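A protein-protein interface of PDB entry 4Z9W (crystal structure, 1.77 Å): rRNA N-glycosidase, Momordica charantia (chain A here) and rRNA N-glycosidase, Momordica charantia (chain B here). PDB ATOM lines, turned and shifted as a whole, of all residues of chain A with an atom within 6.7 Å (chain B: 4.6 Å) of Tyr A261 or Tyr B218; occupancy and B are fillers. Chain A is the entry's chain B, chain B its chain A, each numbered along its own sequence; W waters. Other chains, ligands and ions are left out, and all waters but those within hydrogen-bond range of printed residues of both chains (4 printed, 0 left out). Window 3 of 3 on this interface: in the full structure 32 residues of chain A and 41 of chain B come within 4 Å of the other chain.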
ATOM      1  N   ILE A 137      10.704 -22.654   8.064  1.00  0.00           N
ATOM      2  CA  ILE A 137      10.339 -21.466   8.784  1.00  0.00           C
ATOM      3  C   ILE A 137      10.716 -20.282   7.905  1.00  0.00           C
ATOM      4  O   ILE A 137      11.904 -20.077   7.623  1.00  0.00           O
ATOM      5  CB  ILE A 137      11.037 -21.420  10.137  1.00  0.00           C
ATOM      6  CG1 ILE A 137      10.425 -22.519  11.029  1.00  0.00           C
ATOM      7  CG2 ILE A 137      10.887 -20.060  10.779  1.00  0.00           C
ATOM      8  CD1 ILE A 137      11.408 -23.061  12.005  1.00  0.00           C
ATOM      9  N   VAL A 138       9.715 -19.498   7.536  1.00  0.00           N
ATOM     10  CA  VAL A 138       9.911 -18.311   6.683  1.00  0.00           C
ATOM     11  C   VAL A 138      10.329 -17.107   7.513  1.00  0.00           C
ATOM     12  O   VAL A 138       9.627 -16.759   8.465  1.00  0.00           O
ATOM     13  CB  VAL A 138       8.635 -17.998   5.861  1.00  0.00           C
ATOM     14  CG1 VAL A 138       8.822 -16.755   4.992  1.00  0.00           C
ATOM     15  CG2 VAL A 138       8.260 -19.206   5.008  1.00  0.00           C
ATOM     16  N   THR A 139      11.422 -16.441   7.138  1.00  0.00           N
ATOM     17  CA  THR A 139      12.000 -15.396   7.988  1.00  0.00           C
ATOM     18  C   THR A 139      12.848 -14.419   7.167  1.00  0.00           C
ATOM     19  O   THR A 139      13.246 -14.718   6.023  1.00  0.00           O
ATOM     20  CB  THR A 139      12.884 -16.047   9.091  1.00  0.00           C
ATOM     21  OG1 THR A 139      13.213 -15.098  10.131  1.00  0.00           O
ATOM     22  CG2 THR A 139      14.176 -16.654   8.488  1.00  0.00           C
ATOM     23  N   THR A 140      13.134 -13.276   7.767  1.00  0.00           N
ATOM     24  CA  THR A 140      14.203 -12.406   7.275  1.00  0.00           C
ATOM     25  C   THR A 140      15.390 -12.734   8.150  1.00  0.00           C
ATOM     26  O   THR A 140      15.249 -13.380   9.205  1.00  0.00           O
ATOM     27  CB  THR A 140      13.843 -10.914   7.327  1.00  0.00           C
ATOM     28  OG1 THR A 140      13.603 -10.515   8.685  1.00  0.00           O
ATOM     29  CG2 THR A 140      12.612 -10.626   6.510  1.00  0.00           C
ATOM     30  N   VAL A 259      17.360 -13.709  13.397  1.00  0.00           N
ATOM     31  CA  VAL A 259      16.205 -14.039  12.569  1.00  0.00           C
ATOM     32  C   VAL A 259      15.057 -13.145  12.983  1.00  0.00           C
ATOM     33  O   VAL A 259      14.869 -12.848  14.187  1.00  0.00           O
ATOM     34  CB  VAL A 259      15.810 -15.536  12.654  1.00  0.00           C
ATOM     35  CG1 VAL A 259      16.950 -16.384  12.132  1.00  0.00           C
ATOM     36  CG2 VAL A 259      15.424 -15.952  14.062  1.00  0.00           C
ATOM     37  N   PHE A 260      14.339 -12.655  11.995  1.00  0.00           N
ATOM     38  CA  PHE A 260      13.153 -11.878  12.260  1.00  0.00           C
ATOM     39  C   PHE A 260      12.039 -12.441  11.392  1.00  0.00           C
ATOM     40  O   PHE A 260      11.963 -12.165  10.185  1.00  0.00           O
ATOM     41  CB  PHE A 260      13.320 -10.403  12.012  1.00  0.00           C
ATOM     42  CG  PHE A 260      12.120  -9.642  12.435  1.00  0.00           C
ATOM     43  CD1 PHE A 260      11.914  -9.370  13.777  1.00  0.00           C
ATOM     44  CD2 PHE A 260      11.123  -9.321  11.523  1.00  0.00           C
ATOM     45  CE1 PHE A 260      10.774  -8.712  14.178  1.00  0.00           C
ATOM     46  CE2 PHE A 260       9.960  -8.693  11.926  1.00  0.00           C
ATOM     47  CZ  PHE A 260       9.790  -8.387  13.255  1.00  0.00           C
ATOM     48  N   TYR A 261      11.212 -13.223  12.061  1.00  0.00           N
ATOM     49  CA  TYR A 261      10.202 -14.083  11.455  1.00  0.00           C
ATOM     50  C   TYR A 261       8.835 -13.427  11.764  1.00  0.00           C
ATOM     51  O   TYR A 261       7.800 -14.107  11.501  1.00  0.00           O
ATOM     52  CB  TYR A 261      10.345 -15.506  12.006  1.00  0.00           C
ATOM     53  CG  TYR A 261      10.254 -15.597  13.510  1.00  0.00           C
ATOM     54  CD1 TYR A 261      11.382 -15.414  14.315  1.00  0.00           C
ATOM     55  CD2 TYR A 261       9.037 -15.815  14.125  1.00  0.00           C
ATOM     56  CE1 TYR A 261      11.289 -15.428  15.710  1.00  0.00           C
ATOM     57  CE2 TYR A 261       8.936 -15.833  15.521  1.00  0.00           C
ATOM     58  CZ  TYR A 261      10.056 -15.639  16.299  1.00  0.00           C
ATOM     59  OH  TYR A 261       9.939 -15.693  17.668  1.00  0.00           O
ATOM     60  N   PHE B 166      14.261 -11.175  18.945  1.00  0.00           N
ATOM     61  CA  PHE B 166      13.135 -10.792  18.111  1.00  0.00           C
ATOM     62  C   PHE B 166      12.512  -9.473  18.567  1.00  0.00           C
ATOM     63  O   PHE B 166      12.220  -8.574  17.765  1.00  0.00           O
ATOM     64  CB  PHE B 166      12.109 -11.945  18.088  1.00  0.00           C
ATOM     65  CG  PHE B 166      10.844 -11.628  17.340  1.00  0.00           C
ATOM     66  CD1 PHE B 166       9.788 -10.968  17.957  1.00  0.00           C
ATOM     67  CD2 PHE B 166      10.726 -11.949  15.992  1.00  0.00           C
ATOM     68  CE1 PHE B 166       8.632 -10.669  17.258  1.00  0.00           C
ATOM     69  CE2 PHE B 166       9.563 -11.622  15.285  1.00  0.00           C
ATOM     70  CZ  PHE B 166       8.516 -11.006  15.926  1.00  0.00           C
ATOM     71  N   LEU B 185       1.040 -11.006  18.223  1.00  0.00           N
ATOM     72  CA  LEU B 185       1.100 -12.355  18.791  1.00  0.00           C
ATOM     73  C   LEU B 185       2.505 -12.910  18.847  1.00  0.00           C
ATOM     74  O   LEU B 185       2.814 -13.632  19.778  1.00  0.00           O
ATOM     75  CB  LEU B 185       0.217 -13.329  18.021  1.00  0.00           C
ATOM     76  CG  LEU B 185      -1.282 -12.975  18.003  1.00  0.00           C
ATOM     77  CD1 LEU B 185      -2.022 -14.113  17.365  1.00  0.00           C
ATOM     78  CD2 LEU B 185      -1.863 -12.651  19.383  1.00  0.00           C
ATOM     79  N   ALA B 186       3.325 -12.599  17.833  1.00  0.00           N
ATOM     80  CA  ALA B 186       4.723 -13.052  17.806  1.00  0.00           C
ATOM     81  C   ALA B 186       5.471 -12.587  19.074  1.00  0.00           C
ATOM     82  O   ALA B 186       6.007 -13.413  19.844  1.00  0.00           O
ATOM     83  CB  ALA B 186       5.424 -12.571  16.551  1.00  0.00           C
ATOM     84  N   SER B 189       3.743 -13.924  22.435  1.00  0.00           N
ATOM     85  CA  SER B 189       3.936 -15.329  22.704  1.00  0.00           C
ATOM     86  C   SER B 189       5.332 -15.612  23.284  1.00  0.00           C
ATOM     87  O   SER B 189       5.483 -16.536  24.049  1.00  0.00           O
ATOM     88  CB  SER B 189       3.645 -16.212  21.460  1.00  0.00           C
ATOM     89  OG  SER B 189       4.580 -15.972  20.410  1.00  0.00           O
ATOM     90  N   LEU B 190       6.349 -14.828  22.909  1.00  0.00           N
ATOM     91  CA  LEU B 190       7.666 -14.947  23.494  1.00  0.00           C
ATOM     92  C   LEU B 190       7.635 -14.509  24.988  1.00  0.00           C
ATOM     93  O   LEU B 190       8.047 -15.232  25.877  1.00  0.00           O
ATOM     94  CB  LEU B 190       8.655 -14.076  22.734  1.00  0.00           C
ATOM     95  CG  LEU B 190       8.912 -14.576  21.315  1.00  0.00           C
ATOM     96  CD1 LEU B 190       9.648 -13.499  20.530  1.00  0.00           C
ATOM     97  CD2 LEU B 190       9.707 -15.873  21.300  1.00  0.00           C
ATOM     98  N   SER B 216       3.902 -22.864  21.912  1.00  0.00           N
ATOM     99  CA  SER B 216       3.443 -22.197  20.690  1.00  0.00           C
ATOM    100  C   SER B 216       4.001 -20.788  20.565  1.00  0.00           C
ATOM    101  O   SER B 216       3.653 -19.922  21.360  1.00  0.00           O
ATOM    102  CB  SER B 216       1.915 -22.146  20.577  1.00  0.00           C
ATOM    103  OG  SER B 216       1.409 -23.471  20.467  1.00  0.00           O
ATOM    104  N   LEU B 217       4.866 -20.573  19.578  1.00  0.00           N
ATOM    105  CA  LEU B 217       5.358 -19.235  19.253  1.00  0.00           C
ATOM    106  C   LEU B 217       4.764 -18.780  17.920  1.00  0.00           C
ATOM    107  O   LEU B 217       4.912 -19.470  16.894  1.00  0.00           O
ATOM    108  CB  LEU B 217       6.890 -19.231  19.173  1.00  0.00           C
ATOM    109  CG  LEU B 217       7.617 -19.763  20.394  1.00  0.00           C
ATOM    110  CD1 LEU B 217       9.122 -19.749  20.226  1.00  0.00           C
ATOM    111  CD2 LEU B 217       7.215 -18.897  21.592  1.00  0.00           C
ATOM    112  N   TYR B 218       4.147 -17.607  17.911  1.00  0.00           N
ATOM    113  CA  TYR B 218       3.538 -17.087  16.698  1.00  0.00           C
ATOM    114  C   TYR B 218       4.563 -16.394  15.834  1.00  0.00           C
ATOM    115  O   TYR B 218       5.519 -15.809  16.352  1.00  0.00           O
ATOM    116  CB  TYR B 218       2.430 -16.133  17.082  1.00  0.00           C
ATOM    117  CG  TYR B 218       1.191 -16.892  17.494  1.00  0.00           C
ATOM    118  CD1 TYR B 218       1.100 -17.522  18.749  1.00  0.00           C
ATOM    119  CD2 TYR B 218       0.124 -17.017  16.613  1.00  0.00           C
ATOM    120  CE1 TYR B 218      -0.033 -18.242  19.101  1.00  0.00           C
ATOM    121  CE2 TYR B 218      -1.003 -17.722  16.960  1.00  0.00           C
ATOM    122  CZ  TYR B 218      -1.084 -18.332  18.207  1.00  0.00           C
ATOM    123  OH  TYR B 218      -2.238 -19.059  18.570  1.00  0.00           O
ATOM    124  N   ASN B 219       4.407 -16.498  14.514  1.00  0.00           N
ATOM    125  CA  ASN B 219       5.217 -15.674  13.620  1.00  0.00           C
ATOM    126  C   ASN B 219       4.500 -14.386  13.287  1.00  0.00           C
ATOM    127  O   ASN B 219       3.392 -14.120  13.780  1.00  0.00           O
ATOM    128  CB  ASN B 219       5.646 -16.467  12.385  1.00  0.00           C
ATOM    129  CG  ASN B 219       4.479 -16.816  11.478  1.00  0.00           C
ATOM    130  OD1 ASN B 219       3.366 -16.292  11.629  1.00  0.00           O
ATOM    131  ND2 ASN B 219       4.753 -17.636  10.489  1.00  0.00           N
ATOM    132  N   SER B 220       5.129 -13.552  12.457  1.00  0.00           N
ATOM    133  CA  SER B 220       4.606 -12.233  12.145  1.00  0.00           C
ATOM    134  C   SER B 220       3.340 -12.252  11.275  1.00  0.00           C
ATOM    135  O   SER B 220       2.702 -11.216  11.131  1.00  0.00           O
ATOM    136  CB  SER B 220       5.704 -11.346  11.507  1.00  0.00           C
ATOM    137  OG  SER B 220       6.586 -10.885  12.527  1.00  0.00           O
ATOM    138  N   ASP B 222       0.862 -14.236  12.216  1.00  0.00           N
ATOM    139  CA  ASP B 222      -0.082 -14.792  13.191  1.00  0.00           C
ATOM    140  C   ASP B 222      -0.285 -16.295  13.099  1.00  0.00           C
ATOM    141  O   ASP B 222      -1.324 -16.792  13.561  1.00  0.00           O
ATOM    142  CB  ASP B 222      -1.420 -14.043  13.141  1.00  0.00           C
ATOM    143  CG  ASP B 222      -1.314 -12.634  13.626  1.00  0.00           C
ATOM    144  OD1 ASP B 222      -0.478 -12.346  14.502  1.00  0.00           O
ATOM    145  OD2 ASP B 222      -2.084 -11.785  13.159  1.00  0.00           O
ATOM    146  N   GLU B 223       0.697 -17.025  12.577  1.00  0.00           N
ATOM    147  CA  GLU B 223       0.634 -18.496  12.482  1.00  0.00           C
ATOM    148  C   GLU B 223       1.385 -19.047  13.705  1.00  0.00           C
ATOM    149  O   GLU B 223       2.504 -18.597  14.001  1.00  0.00           O
ATOM    150  CB  GLU B 223       1.306 -19.028  11.191  1.00  0.00           C
ATOM    151  CG  GLU B 223       0.775 -18.435   9.873  1.00  0.00           C
ATOM    152  CD  GLU B 223       1.644 -18.688   8.624  1.00  0.00           C
ATOM    153  OE1 GLU B 223       2.880 -18.830   8.707  1.00  0.00           O
ATOM    154  OE2 GLU B 223       1.077 -18.720   7.511  1.00  0.00           O
ATOM    155  N   PRO B 224       0.787 -20.001  14.433  1.00  0.00           N
ATOM    156  CA  PRO B 224       1.516 -20.602  15.544  1.00  0.00           C
ATOM    157  C   PRO B 224       2.514 -21.643  15.070  1.00  0.00           C
ATOM    158  O   PRO B 224       2.173 -22.501  14.249  1.00  0.00           O
ATOM    159  CB  PRO B 224       0.408 -21.301  16.355  1.00  0.00           C
ATOM    160  CG  PRO B 224      -0.602 -21.674  15.328  1.00  0.00           C
ATOM    161  CD  PRO B 224      -0.591 -20.530  14.343  1.00  0.00           C
ATOM    162  N   ILE B 234      13.913 -20.210  15.579  1.00  0.00           N
ATOM    163  CA  ILE B 234      13.112 -19.142  16.186  1.00  0.00           C
ATOM    164  C   ILE B 234      13.223 -19.112  17.730  1.00  0.00           C
ATOM    165  O   ILE B 234      12.764 -18.167  18.354  1.00  0.00           O
ATOM    166  CB  ILE B 234      11.633 -19.201  15.758  1.00  0.00           C
ATOM    167  CG1 ILE B 234      10.965 -20.472  16.286  1.00  0.00           C
ATOM    168  CG2 ILE B 234      11.522 -19.027  14.248  1.00  0.00           C
ATOM    169  CD1 ILE B 234       9.451 -20.406  16.259  1.00  0.00           C
ATOM    170  N   ASN B 238      17.219 -16.583  19.179  1.00  0.00           N
ATOM    171  CA  ASN B 238      16.282 -15.573  19.603  1.00  0.00           C
ATOM    172  C   ASN B 238      16.368 -15.376  21.132  1.00  0.00           C
ATOM    173  O   ASN B 238      16.767 -14.311  21.601  1.00  0.00           O
ATOM    174  CB  ASN B 238      14.867 -16.010  19.135  1.00  0.00           C
ATOM    175  CG  ASN B 238      13.780 -15.007  19.506  1.00  0.00           C
ATOM    176  OD1 ASN B 238      14.051 -13.935  20.019  1.00  0.00           O
ATOM    177  ND2 ASN B 238      12.547 -15.357  19.241  1.00  0.00           N
HETATM  178  O   HOH W   1      15.228 -13.629  16.866  1.00  0.00           O
HETATM  179  O   HOH W   2       7.243 -15.654  18.523  1.00  0.00           O
HETATM  180  O   HOH W   3       7.715 -17.994  10.192  1.00  0.00           O
HETATM  181  O   HOH W   4       6.114 -14.197   9.453  1.00  0.00           O
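The backbone NH of Phe B166 sits at hydrogen-bond distance from the side-chain amide oxygen of Asn B238.
The side-chain hydroxyl (OG) of Ser B189 sits at hydrogen-bond distance from the backbone NH (N) of Tyr B218 (3.0 Å).
OD1 of Asn B219 is in hydrogen-bond range of N of Asp B222, 3.3 Å away.
The side-chain amide nitrogen (ND2) of Asn B219 lies within hydrogen-bond range of the side-chain carboxylate (OE1) of Glu B223 (2.8 Å).
The side-chain hydroxyl of Thr A139 sits close to the backbone carbonyl oxygen of Phe A260 (3.2 Å).
The backbone carbonyl oxygen (O) of Phe A260 is in hydrogen-bond range of the side-chain hydroxyl (OG1) of Thr A140, 2.8 Å away.
Water W4 bridges O of Tyr A261 and N of Ser B220.
Water W2 lies within hydrogen-bond range of the backbone carbonyl oxygen of Tyr B218, the side-chain hydroxyl of Tyr A261, the backbone carbonyl oxygen of Ala B186 and the side-chain hydroxyl of Ser B189.
Water W1 lies within hydrogen-bond range of the backbone carbonyl oxygen of Val A259, the backbone NH of Phe B166 and the side-chain amide oxygen of Asn B238.
Water W3 lies within hydrogen-bond range of the backbone carbonyl oxygen (O) of Val A138 (2.9 Å) and the side-chain amide nitrogen (ND2) of Asn B219 (3.0 Å).
The backbone NH of Ser B220 lies within hydrogen-bond range of the backbone carbonyl oxygen of Tyr A261 (2.9 Å).
The side-chain hydroxyl (OH) of Tyr A261 is in hydrogen-bond range of the side-chain amide nitrogen (ND2) of Asn B238.
Hydrophobic or aromatic side chains of chain A that line the printed part of chain B: Ile A137, Phe A260 and Tyr A261.
Of the 15 printed residues of chain B, 7 touch a printed residue of chain A.
Hydrophobic or aromatic side chains of chain B that line the printed part of chain A: Phe B166, Leu B190 and Ile B234.
Among the printed residues, 9 pairs touch across the chains.
Among the printed residues, no Asp or Glu carboxylate lies within 4 Å of a Lys or Arg side-chain nitrogen of the other chain.
Among the printed residues, pairs that only touch across the chains: Tyr A261 with Asn B219 (3.3 Å), Phe A260 with Phe B166 (3.3 Å), Tyr A261 with Tyr B218 (3.5 Å), Tyr A261 with Phe B166 (3.5 Å), Tyr A261 with Ile B234 (3.6 Å), Tyr A261 with Leu B190 (3.6 Å) and Ile A137 with Ile B234 (3.7 Å).
Of chain B, only Phe B166, Leu B190, Tyr B218, Asn B219, Ser B220, Ile B234 and Asn B238 come within 4 Å of Tyr A261.
Tyr B218 touches one residue of chain A.
Printed residues of chain A within 4 Å of Ser B220: Tyr A261 (2.9 Å).
Printed residues of chain B within 4 Å of Ile A137: Ile B234 (3.7 Å).
Of the printed residues of chain A, Asn B238 touches Tyr A261.
Of the printed residues of chain A, Leu B190 touches Tyr A261.
Ser B189 touches none of the printed residues of chain A.
The nearest printed residue of chain B that does not touch Tyr A261 is Leu B217 (4.9 Å).
The nearest printed residue of chain A that does not touch Tyr B218 is Ile A137 (8.8 Å).
The nearest printed residue of chain A that does not touch Ser B220 is Phe A260 (4.1 Å).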
